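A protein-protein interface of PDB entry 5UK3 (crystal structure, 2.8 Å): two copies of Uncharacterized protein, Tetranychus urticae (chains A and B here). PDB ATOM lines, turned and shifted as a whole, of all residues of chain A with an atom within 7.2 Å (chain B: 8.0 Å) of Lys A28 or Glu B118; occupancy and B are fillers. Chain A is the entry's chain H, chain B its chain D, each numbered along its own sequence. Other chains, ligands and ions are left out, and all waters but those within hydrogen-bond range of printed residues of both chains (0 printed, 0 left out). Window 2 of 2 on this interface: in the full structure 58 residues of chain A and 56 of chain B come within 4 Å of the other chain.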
ATOM      1  N   ASN A  22      -5.101  -1.304 -19.299  1.00  0.00           N
ATOM      2  CA  ASN A  22      -5.268  -2.244 -18.210  1.00  0.00           C
ATOM      3  C   ASN A  22      -6.635  -2.907 -18.249  1.00  0.00           C
ATOM      4  O   ASN A  22      -6.770  -4.090 -17.948  1.00  0.00           O
ATOM      5  CB  ASN A  22      -5.045  -1.559 -16.864  1.00  0.00           C
ATOM      6  CG  ASN A  22      -4.921  -2.549 -15.722  1.00  0.00           C
ATOM      7  OD1 ASN A  22      -4.445  -3.668 -15.904  1.00  0.00           O
ATOM      8  ND2 ASN A  22      -5.342  -2.136 -14.535  1.00  0.00           N
ATOM      9  N   GLN A  23      -7.652  -2.139 -18.609  1.00  0.00           N
ATOM     10  CA  GLN A  23      -9.005  -2.664 -18.632  1.00  0.00           C
ATOM     11  C   GLN A  23      -9.100  -3.909 -19.492  1.00  0.00           C
ATOM     12  O   GLN A  23      -9.774  -4.864 -19.123  1.00  0.00           O
ATOM     13  CB  GLN A  23      -9.954  -1.604 -19.169  1.00  0.00           C
ATOM     14  CG  GLN A  23      -9.370  -0.814 -20.325  1.00  0.00           C
ATOM     15  CD  GLN A  23     -10.398   0.057 -21.007  1.00  0.00           C
ATOM     16  OE1 GLN A  23     -11.600  -0.177 -20.888  1.00  0.00           O
ATOM     17  NE2 GLN A  23      -9.933   1.065 -21.732  1.00  0.00           N
ATOM     18  N   PHE A  24      -8.429  -3.916 -20.634  1.00  0.00           N
ATOM     19  CA  PHE A  24      -8.464  -5.093 -21.483  1.00  0.00           C
ATOM     20  C   PHE A  24      -7.719  -6.202 -20.756  1.00  0.00           C
ATOM     21  O   PHE A  24      -8.260  -7.279 -20.526  1.00  0.00           O
ATOM     22  CB  PHE A  24      -7.868  -4.787 -22.842  1.00  0.00           C
ATOM     23  CG  PHE A  24      -8.650  -3.772 -23.615  1.00  0.00           C
ATOM     24  CD1 PHE A  24      -9.718  -4.158 -24.399  1.00  0.00           C
ATOM     25  CD2 PHE A  24      -8.330  -2.432 -23.540  1.00  0.00           C
ATOM     26  CE1 PHE A  24     -10.448  -3.226 -25.109  1.00  0.00           C
ATOM     27  CE2 PHE A  24      -9.054  -1.492 -24.247  1.00  0.00           C
ATOM     28  CZ  PHE A  24     -10.115  -1.891 -25.032  1.00  0.00           C
ATOM     29  N   ILE A  25      -6.481  -5.928 -20.376  1.00  0.00           N
ATOM     30  CA  ILE A  25      -5.698  -6.889 -19.603  1.00  0.00           C
ATOM     31  C   ILE A  25      -6.513  -7.514 -18.442  1.00  0.00           C
ATOM     32  O   ILE A  25      -6.461  -8.729 -18.266  1.00  0.00           O
ATOM     33  CB  ILE A  25      -4.362  -6.318 -19.051  1.00  0.00           C
ATOM     34  CG1 ILE A  25      -3.425  -5.892 -20.199  1.00  0.00           C
ATOM     35  CG2 ILE A  25      -3.658  -7.360 -18.174  1.00  0.00           C
ATOM     36  CD1 ILE A  25      -2.236  -5.045 -19.747  1.00  0.00           C
ATOM     37  N   LYS A  26      -7.248  -6.701 -17.692  1.00  0.00           N
ATOM     38  CA  LYS A  26      -8.009  -7.204 -16.554  1.00  0.00           C
ATOM     39  C   LYS A  26      -9.020  -8.232 -17.032  1.00  0.00           C
ATOM     40  O   LYS A  26      -9.173  -9.292 -16.437  1.00  0.00           O
ATOM     41  CB  LYS A  26      -8.713  -6.041 -15.860  1.00  0.00           C
ATOM     42  CG  LYS A  26      -8.814  -6.167 -14.352  1.00  0.00           C
ATOM     43  CD  LYS A  26      -9.463  -4.929 -13.755  1.00  0.00           C
ATOM     44  CE  LYS A  26      -9.628  -5.057 -12.250  1.00  0.00           C
ATOM     45  NZ  LYS A  26     -10.414  -3.932 -11.672  1.00  0.00           N
ATOM     46  N   ALA A  27      -9.685  -7.914 -18.128  1.00  0.00           N
ATOM     47  CA  ALA A  27     -10.644  -8.805 -18.786  1.00  0.00           C
ATOM     48  C   ALA A  27     -10.019 -10.112 -19.244  1.00  0.00           C
ATOM     49  O   ALA A  27     -10.622 -11.182 -19.080  1.00  0.00           O
ATOM     50  CB  ALA A  27     -11.293  -8.099 -19.973  1.00  0.00           C
ATOM     51  N   LYS A  28      -8.812 -10.028 -19.803  1.00  0.00           N
ATOM     52  CA  LYS A  28      -8.047 -11.221 -20.214  1.00  0.00           C
ATOM     53  C   LYS A  28      -7.669 -12.164 -19.057  1.00  0.00           C
ATOM     54  O   LYS A  28      -7.822 -13.389 -19.198  1.00  0.00           O
ATOM     55  CB  LYS A  28      -6.771 -10.830 -20.950  1.00  0.00           C
ATOM     56  CG  LYS A  28      -5.984 -12.038 -21.459  1.00  0.00           C
ATOM     57  CD  LYS A  28      -4.729 -11.670 -22.181  1.00  0.00           C
ATOM     58  CE  LYS A  28      -3.589 -11.040 -21.360  1.00  0.00           C
ATOM     59  NZ  LYS A  28      -2.844 -11.745 -20.279  1.00  0.00           N
ATOM     60  N   GLU A  29      -7.227 -11.598 -17.927  1.00  0.00           N
ATOM     61  CA  GLU A  29      -6.865 -12.374 -16.731  1.00  0.00           C
ATOM     62  C   GLU A  29      -8.071 -13.141 -16.131  1.00  0.00           C
ATOM     63  O   GLU A  29      -7.954 -14.339 -15.859  1.00  0.00           O
ATOM     64  CB  GLU A  29      -6.115 -11.502 -15.681  1.00  0.00           C
ATOM     65  CG  GLU A  29      -4.735 -11.062 -16.190  1.00  0.00           C
ATOM     66  CD  GLU A  29      -3.894 -10.145 -15.316  1.00  0.00           C
ATOM     67  OE1 GLU A  29      -4.446  -9.627 -14.294  1.00  0.00           O
ATOM     68  OE2 GLU A  29      -2.718  -9.891 -15.667  1.00  0.00           O
ATOM     69  N   SER A  30      -9.231 -12.484 -16.038  1.00  0.00           N
ATOM     70  CA  SER A  30     -10.514 -13.124 -15.658  1.00  0.00           C
ATOM     71  C   SER A  30     -10.834 -14.394 -16.412  1.00  0.00           C
ATOM     72  O   SER A  30     -11.220 -15.397 -15.809  1.00  0.00           O
ATOM     73  CB  SER A  30     -11.691 -12.172 -15.878  1.00  0.00           C
ATOM     74  OG  SER A  30     -11.722 -11.162 -14.897  1.00  0.00           O
ATOM     75  N   LYS A  31     -10.723 -14.329 -17.733  1.00  0.00           N
ATOM     76  CA  LYS A  31     -11.032 -15.471 -18.604  1.00  0.00           C
ATOM     77  C   LYS A  31      -9.977 -16.590 -18.589  1.00  0.00           C
ATOM     78  O   LYS A  31     -10.245 -17.688 -19.097  1.00  0.00           O
ATOM     79  CB  LYS A  31     -11.248 -14.997 -20.057  1.00  0.00           C
ATOM     80  CG  LYS A  31     -12.387 -14.008 -20.249  1.00  0.00           C
ATOM     81  CD  LYS A  31     -13.721 -14.709 -20.136  1.00  0.00           C
ATOM     82  CE  LYS A  31     -14.842 -13.683 -19.932  1.00  0.00           C
ATOM     83  NZ  LYS A  31     -16.298 -14.078 -20.058  1.00  0.00           N
ATOM     84  N   GLY A  32      -8.789 -16.311 -18.044  1.00  0.00           N
ATOM     85  CA  GLY A  32      -7.681 -17.271 -18.048  1.00  0.00           C
ATOM     86  C   GLY A  32      -7.054 -17.460 -19.423  1.00  0.00           C
ATOM     87  O   GLY A  32      -6.511 -18.523 -19.721  1.00  0.00           O
ATOM     88  N   LEU A  33      -7.146 -16.428 -20.268  1.00  0.00           N
ATOM     89  CA  LEU A  33      -6.585 -16.457 -21.624  1.00  0.00           C
ATOM     90  C   LEU A  33      -5.108 -16.066 -21.641  1.00  0.00           C
ATOM     91  O   LEU A  33      -4.711 -15.109 -20.981  1.00  0.00           O
ATOM     92  CB  LEU A  33      -7.355 -15.489 -22.522  1.00  0.00           C
ATOM     93  CG  LEU A  33      -8.674 -15.973 -23.090  1.00  0.00           C
ATOM     94  CD1 LEU A  33      -9.464 -14.793 -23.642  1.00  0.00           C
ATOM     95  CD2 LEU A  33      -8.439 -17.009 -24.187  1.00  0.00           C
ATOM     96  N   THR A  34      -4.300 -16.778 -22.415  1.00  0.00           N
ATOM     97  CA  THR A  34      -2.916 -16.364 -22.656  1.00  0.00           C
ATOM     98  C   THR A  34      -2.861 -15.511 -23.901  1.00  0.00           C
ATOM     99  O   THR A  34      -3.764 -15.586 -24.747  1.00  0.00           O
ATOM    100  CB  THR A  34      -1.973 -17.565 -22.829  1.00  0.00           C
ATOM    101  OG1 THR A  34      -2.400 -18.372 -23.924  1.00  0.00           O
ATOM    102  CG2 THR A  34      -1.951 -18.417 -21.554  1.00  0.00           C
ATOM    103  N   TYR A  35      -1.819 -14.689 -24.019  1.00  0.00           N
ATOM    104  CA  TYR A  35      -1.608 -13.881 -25.216  1.00  0.00           C
ATOM    105  C   TYR A  35      -1.497 -14.807 -26.436  1.00  0.00           C
ATOM    106  O   TYR A  35      -2.062 -14.525 -27.484  1.00  0.00           O
ATOM    107  CB  TYR A  35      -0.359 -12.998 -25.100  1.00  0.00           C
ATOM    108  CG  TYR A  35      -0.444 -11.887 -24.064  1.00  0.00           C
ATOM    109  CD1 TYR A  35      -1.242 -10.772 -24.258  1.00  0.00           C
ATOM    110  CD2 TYR A  35       0.303 -11.953 -22.886  1.00  0.00           C
ATOM    111  CE1 TYR A  35      -1.314  -9.768 -23.303  1.00  0.00           C
ATOM    112  CE2 TYR A  35       0.242 -10.956 -21.933  1.00  0.00           C
ATOM    113  CZ  TYR A  35      -0.561  -9.872 -22.137  1.00  0.00           C
ATOM    114  OH  TYR A  35      -0.621  -8.873 -21.175  1.00  0.00           O
ATOM    115  N   GLN A  36      -0.779 -15.919 -26.284  1.00  0.00           N
ATOM    116  CA  GLN A  36      -0.710 -16.975 -27.314  1.00  0.00           C
ATOM    117  C   GLN A  36      -2.098 -17.408 -27.818  1.00  0.00           C
ATOM    118  O   GLN A  36      -2.354 -17.410 -29.018  1.00  0.00           O
ATOM    119  CB  GLN A  36       0.040 -18.184 -26.740  1.00  0.00           C
ATOM    120  CG  GLN A  36       0.215 -19.373 -27.677  1.00  0.00           C
ATOM    121  CD  GLN A  36       1.170 -19.064 -28.799  1.00  0.00           C
ATOM    122  OE1 GLN A  36       2.387 -19.239 -28.657  1.00  0.00           O
ATOM    123  NE2 GLN A  36       0.629 -18.590 -29.923  1.00  0.00           N
ATOM    124  N   GLN A  37      -2.966 -17.778 -26.888  1.00  0.00           N
ATOM    125  CA  GLN A  37      -4.304 -18.239 -27.221  1.00  0.00           C
ATOM    126  C   GLN A  37      -5.088 -17.193 -27.983  1.00  0.00           C
ATOM    127  O   GLN A  37      -5.679 -17.498 -29.016  1.00  0.00           O
ATOM    128  CB  GLN A  37      -5.084 -18.628 -25.965  1.00  0.00           C
ATOM    129  CG  GLN A  37      -4.686 -19.988 -25.390  1.00  0.00           C
ATOM    130  CD  GLN A  37      -5.088 -20.187 -23.929  1.00  0.00           C
ATOM    131  OE1 GLN A  37      -5.770 -19.354 -23.321  1.00  0.00           O
ATOM    132  NE2 GLN A  37      -4.667 -21.310 -23.361  1.00  0.00           N
ATOM    133  N   MET A  38      -5.078 -15.959 -27.489  1.00  0.00           N
ATOM    134  CA  MET A  38      -5.796 -14.878 -28.157  1.00  0.00           C
ATOM    135  C   MET A  38      -5.328 -14.664 -29.587  1.00  0.00           C
ATOM    136  O   MET A  38      -6.130 -14.437 -30.482  1.00  0.00           O
ATOM    137  CB  MET A  38      -5.631 -13.581 -27.393  1.00  0.00           C
ATOM    138  CG  MET A  38      -6.420 -13.541 -26.104  1.00  0.00           C
ATOM    139  SD  MET A  38      -6.338 -11.902 -25.375  1.00  0.00           S
ATOM    140  CE  MET A  38      -7.302 -10.900 -26.522  1.00  0.00           C
ATOM    141  N   LYS A  46       1.239 -12.571 -32.334  1.00  0.00           N
ATOM    142  CA  LYS A  46       1.107 -12.505 -30.876  1.00  0.00           C
ATOM    143  C   LYS A  46       1.620 -11.198 -30.253  1.00  0.00           C
ATOM    144  O   LYS A  46       0.929 -10.600 -29.423  1.00  0.00           O
ATOM    145  CB  LYS A  46       1.854 -13.666 -30.239  1.00  0.00           C
ATOM    146  CG  LYS A  46       1.501 -13.901 -28.786  1.00  0.00           C
ATOM    147  CD  LYS A  46       2.712 -14.329 -27.982  1.00  0.00           C
ATOM    148  CE  LYS A  46       3.271 -15.660 -28.434  1.00  0.00           C
ATOM    149  NZ  LYS A  46       4.530 -15.915 -27.683  1.00  0.00           N
ATOM    150  N   THR A  50      -0.557  -8.136 -28.529  1.00  0.00           N
ATOM    151  CA  THR A  50      -0.241  -7.763 -27.174  1.00  0.00           C
ATOM    152  C   THR A  50      -0.034  -6.260 -27.097  1.00  0.00           C
ATOM    153  O   THR A  50      -0.607  -5.599 -26.237  1.00  0.00           O
ATOM    154  CB  THR A  50       1.000  -8.529 -26.661  1.00  0.00           C
ATOM    155  OG1 THR A  50       0.756  -9.932 -26.765  1.00  0.00           O
ATOM    156  CG2 THR A  50       1.279  -8.198 -25.195  1.00  0.00           C
ATOM    157  N   LEU A  53      -3.373  -4.351 -27.175  1.00  0.00           N
ATOM    158  CA  LEU A  53      -3.991  -4.370 -25.852  1.00  0.00           C
ATOM    159  C   LEU A  53      -3.285  -3.447 -24.863  1.00  0.00           C
ATOM    160  O   LEU A  53      -3.941  -2.834 -24.028  1.00  0.00           O
ATOM    161  CB  LEU A  53      -4.010  -5.778 -25.283  1.00  0.00           C
ATOM    162  CG  LEU A  53      -4.715  -6.850 -26.087  1.00  0.00           C
ATOM    163  CD1 LEU A  53      -4.503  -8.177 -25.413  1.00  0.00           C
ATOM    164  CD2 LEU A  53      -6.211  -6.537 -26.206  1.00  0.00           C
ATOM    165  N   HIS A  54      -1.962  -3.309 -24.971  1.00  0.00           N
ATOM    166  CA  HIS A  54      -1.214  -2.366 -24.103  1.00  0.00           C
ATOM    167  C   HIS A  54      -1.267  -0.902 -24.570  1.00  0.00           C
ATOM    168  O   HIS A  54      -0.742  -0.036 -23.886  1.00  0.00           O
ATOM    169  CB  HIS A  54       0.241  -2.788 -23.950  1.00  0.00           C
ATOM    170  CG  HIS A  54       0.430  -3.986 -23.100  1.00  0.00           C
ATOM    171  ND1 HIS A  54      -0.112  -5.223 -23.396  1.00  0.00           N
ATOM    172  CD2 HIS A  54       1.081  -4.136 -21.936  1.00  0.00           C
ATOM    173  CE1 HIS A  54       0.208  -6.087 -22.452  1.00  0.00           C
ATOM    174  NE2 HIS A  54       0.927  -5.450 -21.553  1.00  0.00           N
ATOM    175  N   LEU A  71     -12.621 -11.403 -25.327  1.00  0.00           N
ATOM    176  CA  LEU A  71     -12.609 -11.021 -23.929  1.00  0.00           C
ATOM    177  C   LEU A  71     -14.052 -10.917 -23.453  1.00  0.00           C
ATOM    178  O   LEU A  71     -14.996 -11.028 -24.255  1.00  0.00           O
ATOM    179  CB  LEU A  71     -11.887  -9.676 -23.771  1.00  0.00           C
ATOM    180  CG  LEU A  71     -10.426  -9.640 -24.268  1.00  0.00           C
ATOM    181  CD1 LEU A  71      -9.862  -8.229 -24.313  1.00  0.00           C
ATOM    182  CD2 LEU A  71      -9.515 -10.528 -23.415  1.00  0.00           C
ATOM    183  N   GLY A  72     -14.257 -10.683 -22.161  1.00  0.00           N
ATOM    184  CA  GLY A  72     -15.629 -10.488 -21.673  1.00  0.00           C
ATOM    185  C   GLY A  72     -16.402  -9.292 -22.244  1.00  0.00           C
ATOM    186  O   GLY A  72     -17.617  -9.288 -22.237  1.00  0.00           O
ATOM    187  N   ILE A  73     -15.688  -8.291 -22.752  1.00  0.00           N
ATOM    188  CA  ILE A  73     -16.166  -6.902 -22.769  1.00  0.00           C
ATOM    189  C   ILE A  73     -17.124  -6.495 -23.893  1.00  0.00           C
ATOM    190  O   ILE A  73     -17.250  -7.168 -24.909  1.00  0.00           O
ATOM    191  CB  ILE A  73     -14.979  -5.898 -22.751  1.00  0.00           C
ATOM    192  CG1 ILE A  73     -14.088  -6.076 -23.978  1.00  0.00           C
ATOM    193  CG2 ILE A  73     -14.144  -6.051 -21.488  1.00  0.00           C
ATOM    194  CD1 ILE A  73     -13.067  -4.984 -24.092  1.00  0.00           C
ATOM    195  N   SER B 111       5.073  -5.258 -23.986  1.00  0.00           N
ATOM    196  CA  SER B 111       4.457  -6.462 -24.548  1.00  0.00           C
ATOM    197  C   SER B 111       5.369  -7.654 -24.373  1.00  0.00           C
ATOM    198  O   SER B 111       4.936  -8.732 -23.989  1.00  0.00           O
ATOM    199  CB  SER B 111       4.145  -6.268 -26.041  1.00  0.00           C
ATOM    200  OG  SER B 111       3.265  -5.198 -26.218  1.00  0.00           O
ATOM    201  N   LEU B 112       6.624  -7.458 -24.686  1.00  0.00           N
ATOM    202  CA  LEU B 112       7.605  -8.504 -24.475  1.00  0.00           C
ATOM    203  C   LEU B 112       7.732  -8.881 -23.004  1.00  0.00           C
ATOM    204  O   LEU B 112       7.883 -10.049 -22.660  1.00  0.00           O
ATOM    205  CB  LEU B 112       8.960  -8.065 -25.018  1.00  0.00           C
ATOM    206  CG  LEU B 112       8.954  -7.936 -26.553  1.00  0.00           C
ATOM    207  CD1 LEU B 112      10.224  -7.234 -27.014  1.00  0.00           C
ATOM    208  CD2 LEU B 112       8.835  -9.300 -27.222  1.00  0.00           C
ATOM    209  N   ARG B 113       7.634  -7.886 -22.127  1.00  0.00           N
ATOM    210  CA  ARG B 113       7.698  -8.154 -20.699  1.00  0.00           C
ATOM    211  C   ARG B 113       6.518  -9.011 -20.268  1.00  0.00           C
ATOM    212  O   ARG B 113       6.687  -9.992 -19.555  1.00  0.00           O
ATOM    213  CB  ARG B 113       7.718  -6.860 -19.900  1.00  0.00           C
ATOM    214  CG  ARG B 113       7.722  -7.092 -18.404  1.00  0.00           C
ATOM    215  CD  ARG B 113       8.032  -5.830 -17.636  1.00  0.00           C
ATOM    216  NE  ARG B 113       7.162  -4.733 -18.026  1.00  0.00           N
ATOM    217  CZ  ARG B 113       6.936  -3.664 -17.275  1.00  0.00           C
ATOM    218  NH1 ARG B 113       6.132  -2.707 -17.706  1.00  0.00           N
ATOM    219  NH2 ARG B 113       7.508  -3.557 -16.088  1.00  0.00           N
ATOM    220  N   GLY B 114       5.322  -8.660 -20.730  1.00  0.00           N
ATOM    221  CA  GLY B 114       4.127  -9.452 -20.432  1.00  0.00           C
ATOM    222  C   GLY B 114       4.124 -10.865 -20.984  1.00  0.00           C
ATOM    223  O   GLY B 114       3.767 -11.816 -20.260  1.00  0.00           O
ATOM    224  N   ILE B 115       4.570 -11.017 -22.227  1.00  0.00           N
ATOM    225  CA  ILE B 115       4.656 -12.330 -22.819  1.00  0.00           C
ATOM    226  C   ILE B 115       5.686 -13.192 -22.102  1.00  0.00           C
ATOM    227  O   ILE B 115       5.396 -14.353 -21.798  1.00  0.00           O
ATOM    228  CB  ILE B 115       4.995 -12.277 -24.315  1.00  0.00           C
ATOM    229  CG1 ILE B 115       3.815 -11.684 -25.085  1.00  0.00           C
ATOM    230  CG2 ILE B 115       5.273 -13.682 -24.845  1.00  0.00           C
ATOM    231  CD1 ILE B 115       4.223 -11.127 -26.421  1.00  0.00           C
ATOM    232  N   ILE B 116       6.852 -12.629 -21.809  1.00  0.00           N
ATOM    233  CA  ILE B 116       7.886 -13.405 -21.161  1.00  0.00           C
ATOM    234  C   ILE B 116       7.426 -13.819 -19.772  1.00  0.00           C
ATOM    235  O   ILE B 116       7.703 -14.951 -19.339  1.00  0.00           O
ATOM    236  CB  ILE B 116       9.226 -12.667 -21.124  1.00  0.00           C
ATOM    237  CG1 ILE B 116       9.829 -12.632 -22.519  1.00  0.00           C
ATOM    238  CG2 ILE B 116      10.222 -13.407 -20.241  1.00  0.00           C
ATOM    239  CD1 ILE B 116      10.917 -11.596 -22.699  1.00  0.00           C
ATOM    240  N   HIS B 117       6.739 -12.922 -19.063  1.00  0.00           N
ATOM    241  CA  HIS B 117       6.269 -13.273 -17.731  1.00  0.00           C
ATOM    242  C   HIS B 117       5.296 -14.416 -17.740  1.00  0.00           C
ATOM    243  O   HIS B 117       5.384 -15.314 -16.905  1.00  0.00           O
ATOM    244  CB  HIS B 117       5.626 -12.107 -17.001  1.00  0.00           C
ATOM    245  CG  HIS B 117       6.605 -11.091 -16.531  1.00  0.00           C
ATOM    246  ND1 HIS B 117       6.260  -9.817 -16.129  1.00  0.00           N
ATOM    247  CD2 HIS B 117       7.941 -11.184 -16.381  1.00  0.00           C
ATOM    248  CE1 HIS B 117       7.356  -9.162 -15.779  1.00  0.00           C
ATOM    249  NE2 HIS B 117       8.388  -9.969 -15.926  1.00  0.00           N
ATOM    250  N   GLU B 118       4.355 -14.366 -18.670  1.00  0.00           N
ATOM    251  CA  GLU B 118       3.323 -15.389 -18.809  1.00  0.00           C
ATOM    252  C   GLU B 118       3.895 -16.726 -19.253  1.00  0.00           C
ATOM    253  O   GLU B 118       3.556 -17.748 -18.682  1.00  0.00           O
ATOM    254  CB  GLU B 118       2.286 -14.900 -19.785  1.00  0.00           C
ATOM    255  CG  GLU B 118       1.365 -15.943 -20.332  1.00  0.00           C
ATOM    256  CD  GLU B 118       0.296 -15.300 -21.165  1.00  0.00           C
ATOM    257  OE1 GLU B 118       0.376 -15.390 -22.438  1.00  0.00           O
ATOM    258  OE2 GLU B 118      -0.634 -14.698 -20.544  1.00  0.00           O
ATOM    259  N   GLU B 119       4.830 -16.732 -20.199  1.00  0.00           N
ATOM    260  CA  GLU B 119       5.371 -17.986 -20.760  1.00  0.00           C
ATOM    261  C   GLU B 119       6.627 -18.572 -20.065  1.00  0.00           C
ATOM    262  O   GLU B 119       6.898 -19.737 -20.240  1.00  0.00           O
ATOM    263  CB  GLU B 119       5.658 -17.787 -22.245  1.00  0.00           C
ATOM    264  CG  GLU B 119       4.444 -17.318 -23.032  1.00  0.00           C
ATOM    265  CD  GLU B 119       4.650 -17.305 -24.538  1.00  0.00           C
ATOM    266  OE1 GLU B 119       5.749 -17.699 -25.022  1.00  0.00           O
ATOM    267  OE2 GLU B 119       3.700 -16.901 -25.263  1.00  0.00           O
ATOM    268  N   PHE B 120       7.421 -17.757 -19.374  1.00  0.00           N
ATOM    269  CA  PHE B 120       8.603 -18.245 -18.648  1.00  0.00           C
ATOM    270  C   PHE B 120       8.511 -18.073 -17.150  1.00  0.00           C
ATOM    271  O   PHE B 120       9.121 -18.843 -16.398  1.00  0.00           O
ATOM    272  CB  PHE B 120       9.860 -17.515 -19.085  1.00  0.00           C
ATOM    273  CG  PHE B 120      10.226 -17.734 -20.513  1.00  0.00           C
ATOM    274  CD1 PHE B 120       9.606 -17.001 -21.518  1.00  0.00           C
ATOM    275  CD2 PHE B 120      11.214 -18.648 -20.858  1.00  0.00           C
ATOM    276  CE1 PHE B 120       9.974 -17.167 -22.835  1.00  0.00           C
ATOM    277  CE2 PHE B 120      11.567 -18.832 -22.173  1.00  0.00           C
ATOM    278  CZ  PHE B 120      10.963 -18.075 -23.164  1.00  0.00           C
ATOM    279  N   GLY B 121       7.824 -17.032 -16.699  1.00  0.00           N
ATOM    280  CA  GLY B 121       7.721 -16.746 -15.283  1.00  0.00           C
ATOM    281  C   GLY B 121       8.426 -15.451 -14.950  1.00  0.00           C
ATOM    282  O   GLY B 121       8.804 -14.666 -15.832  1.00  0.00           O
ATOM    283  N   ASP B 122       8.603 -15.224 -13.663  1.00  0.00           N
ATOM    284  CA  ASP B 122       9.205 -14.007 -13.191  1.00  0.00           C
ATOM    285  C   ASP B 122      10.715 -14.097 -13.318  1.00  0.00           C
ATOM    286  O   ASP B 122      11.409 -14.683 -12.486  1.00  0.00           O
ATOM    287  CB  ASP B 122       8.818 -13.794 -11.745  1.00  0.00           C
ATOM    288  CG  ASP B 122       9.427 -12.565 -11.169  1.00  0.00           C
ATOM    289  OD1 ASP B 122       9.810 -11.630 -11.955  1.00  0.00           O
ATOM    290  OD2 ASP B 122       9.499 -12.492  -9.906  1.00  0.00           O
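OE2 of Glu B118 lies within salt-bridge range of NZ of Lys A28, at 3.7 Å.
The backbone NH (N) of Tyr A35 is in hydrogen-bond range of the side-chain carboxylate (OE1) of Glu B118, at 2.8 Å.
The side-chain carboxylate (OE2) of Glu B119 is in salt-bridge range of the side-chain amino group (NZ) of Lys A46, 2.7 Å away.
The backbone carbonyl oxygen (O) of Lys A28 is in hydrogen-bond range of the backbone NH (N) of Leu A33 (3.3 Å).
The backbone NH (N) of Gln A37 lies within hydrogen-bond range of the side-chain hydroxyl (OG1) of Thr A34 (3.1 Å).
The backbone carbonyl oxygen (O) of Lys A46 sits at hydrogen-bond distance from the side-chain hydroxyl (OG1) of Thr A50.
A ring nitrogen (ND1) of His A54 is in hydrogen-bond range of the backbone carbonyl oxygen (O) of Thr A50 (2.9 Å).
Among the printed residues, pairs that only touch across the chains: Thr A34 with Glu B118, Thr A50 with Ser B111, Thr A50 with Ile B115, Lys A46 with Ile B115 and Tyr A35 with Gly B114.
Of chain B, only Glu B118 (3.7 Å) comes within 4 Å of Lys A28.
Glu B118 touches just these residues of chain A: Lys A28 (3.7 Å), Thr A34 (3.2 Å) and Tyr A35 (2.8 Å).
No residue of chain B comes within 4 Å of Ala A27.
Of the printed residues of chain A, Ile B115 touches Lys A46 and Thr A50.
Printed residues of chain B within 4 Å of Thr A50: Ser B111 and Ile B115.
Of the printed residues of chain B, Thr A34 touches Glu B118.
The nearest residue of chain A that does not touch Glu B118 is Gln A36 (4.1 Å).
The nearest printed residue of chain A that does not touch Ile B115 is Tyr A35 (4.2 Å).
Of the 24 printed residues of chain A, 5 touch a printed residue of chain B.
Hydrophobic or aromatic side chains of chain A within 4 Å of the printed part of chain B: Tyr A35.
Of the 12 printed residues of chain B, 5 touch a printed residue of chain A.
Printed residues of chain B that touch a printed residue of chain A: Ser B111, Gly B114, Ile B115, Glu B118 and Glu B119.
Hydrophobic or aromatic side chains of chain B within 4 Å of the printed part of chain A: Ile B115.
Among the printed residues, 8 pairs touch across the chains.
No position is printed for both chains.
Of the 8 pairs that touch across the chains among the printed residues, none has its exchanged pair printed and touching as well.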
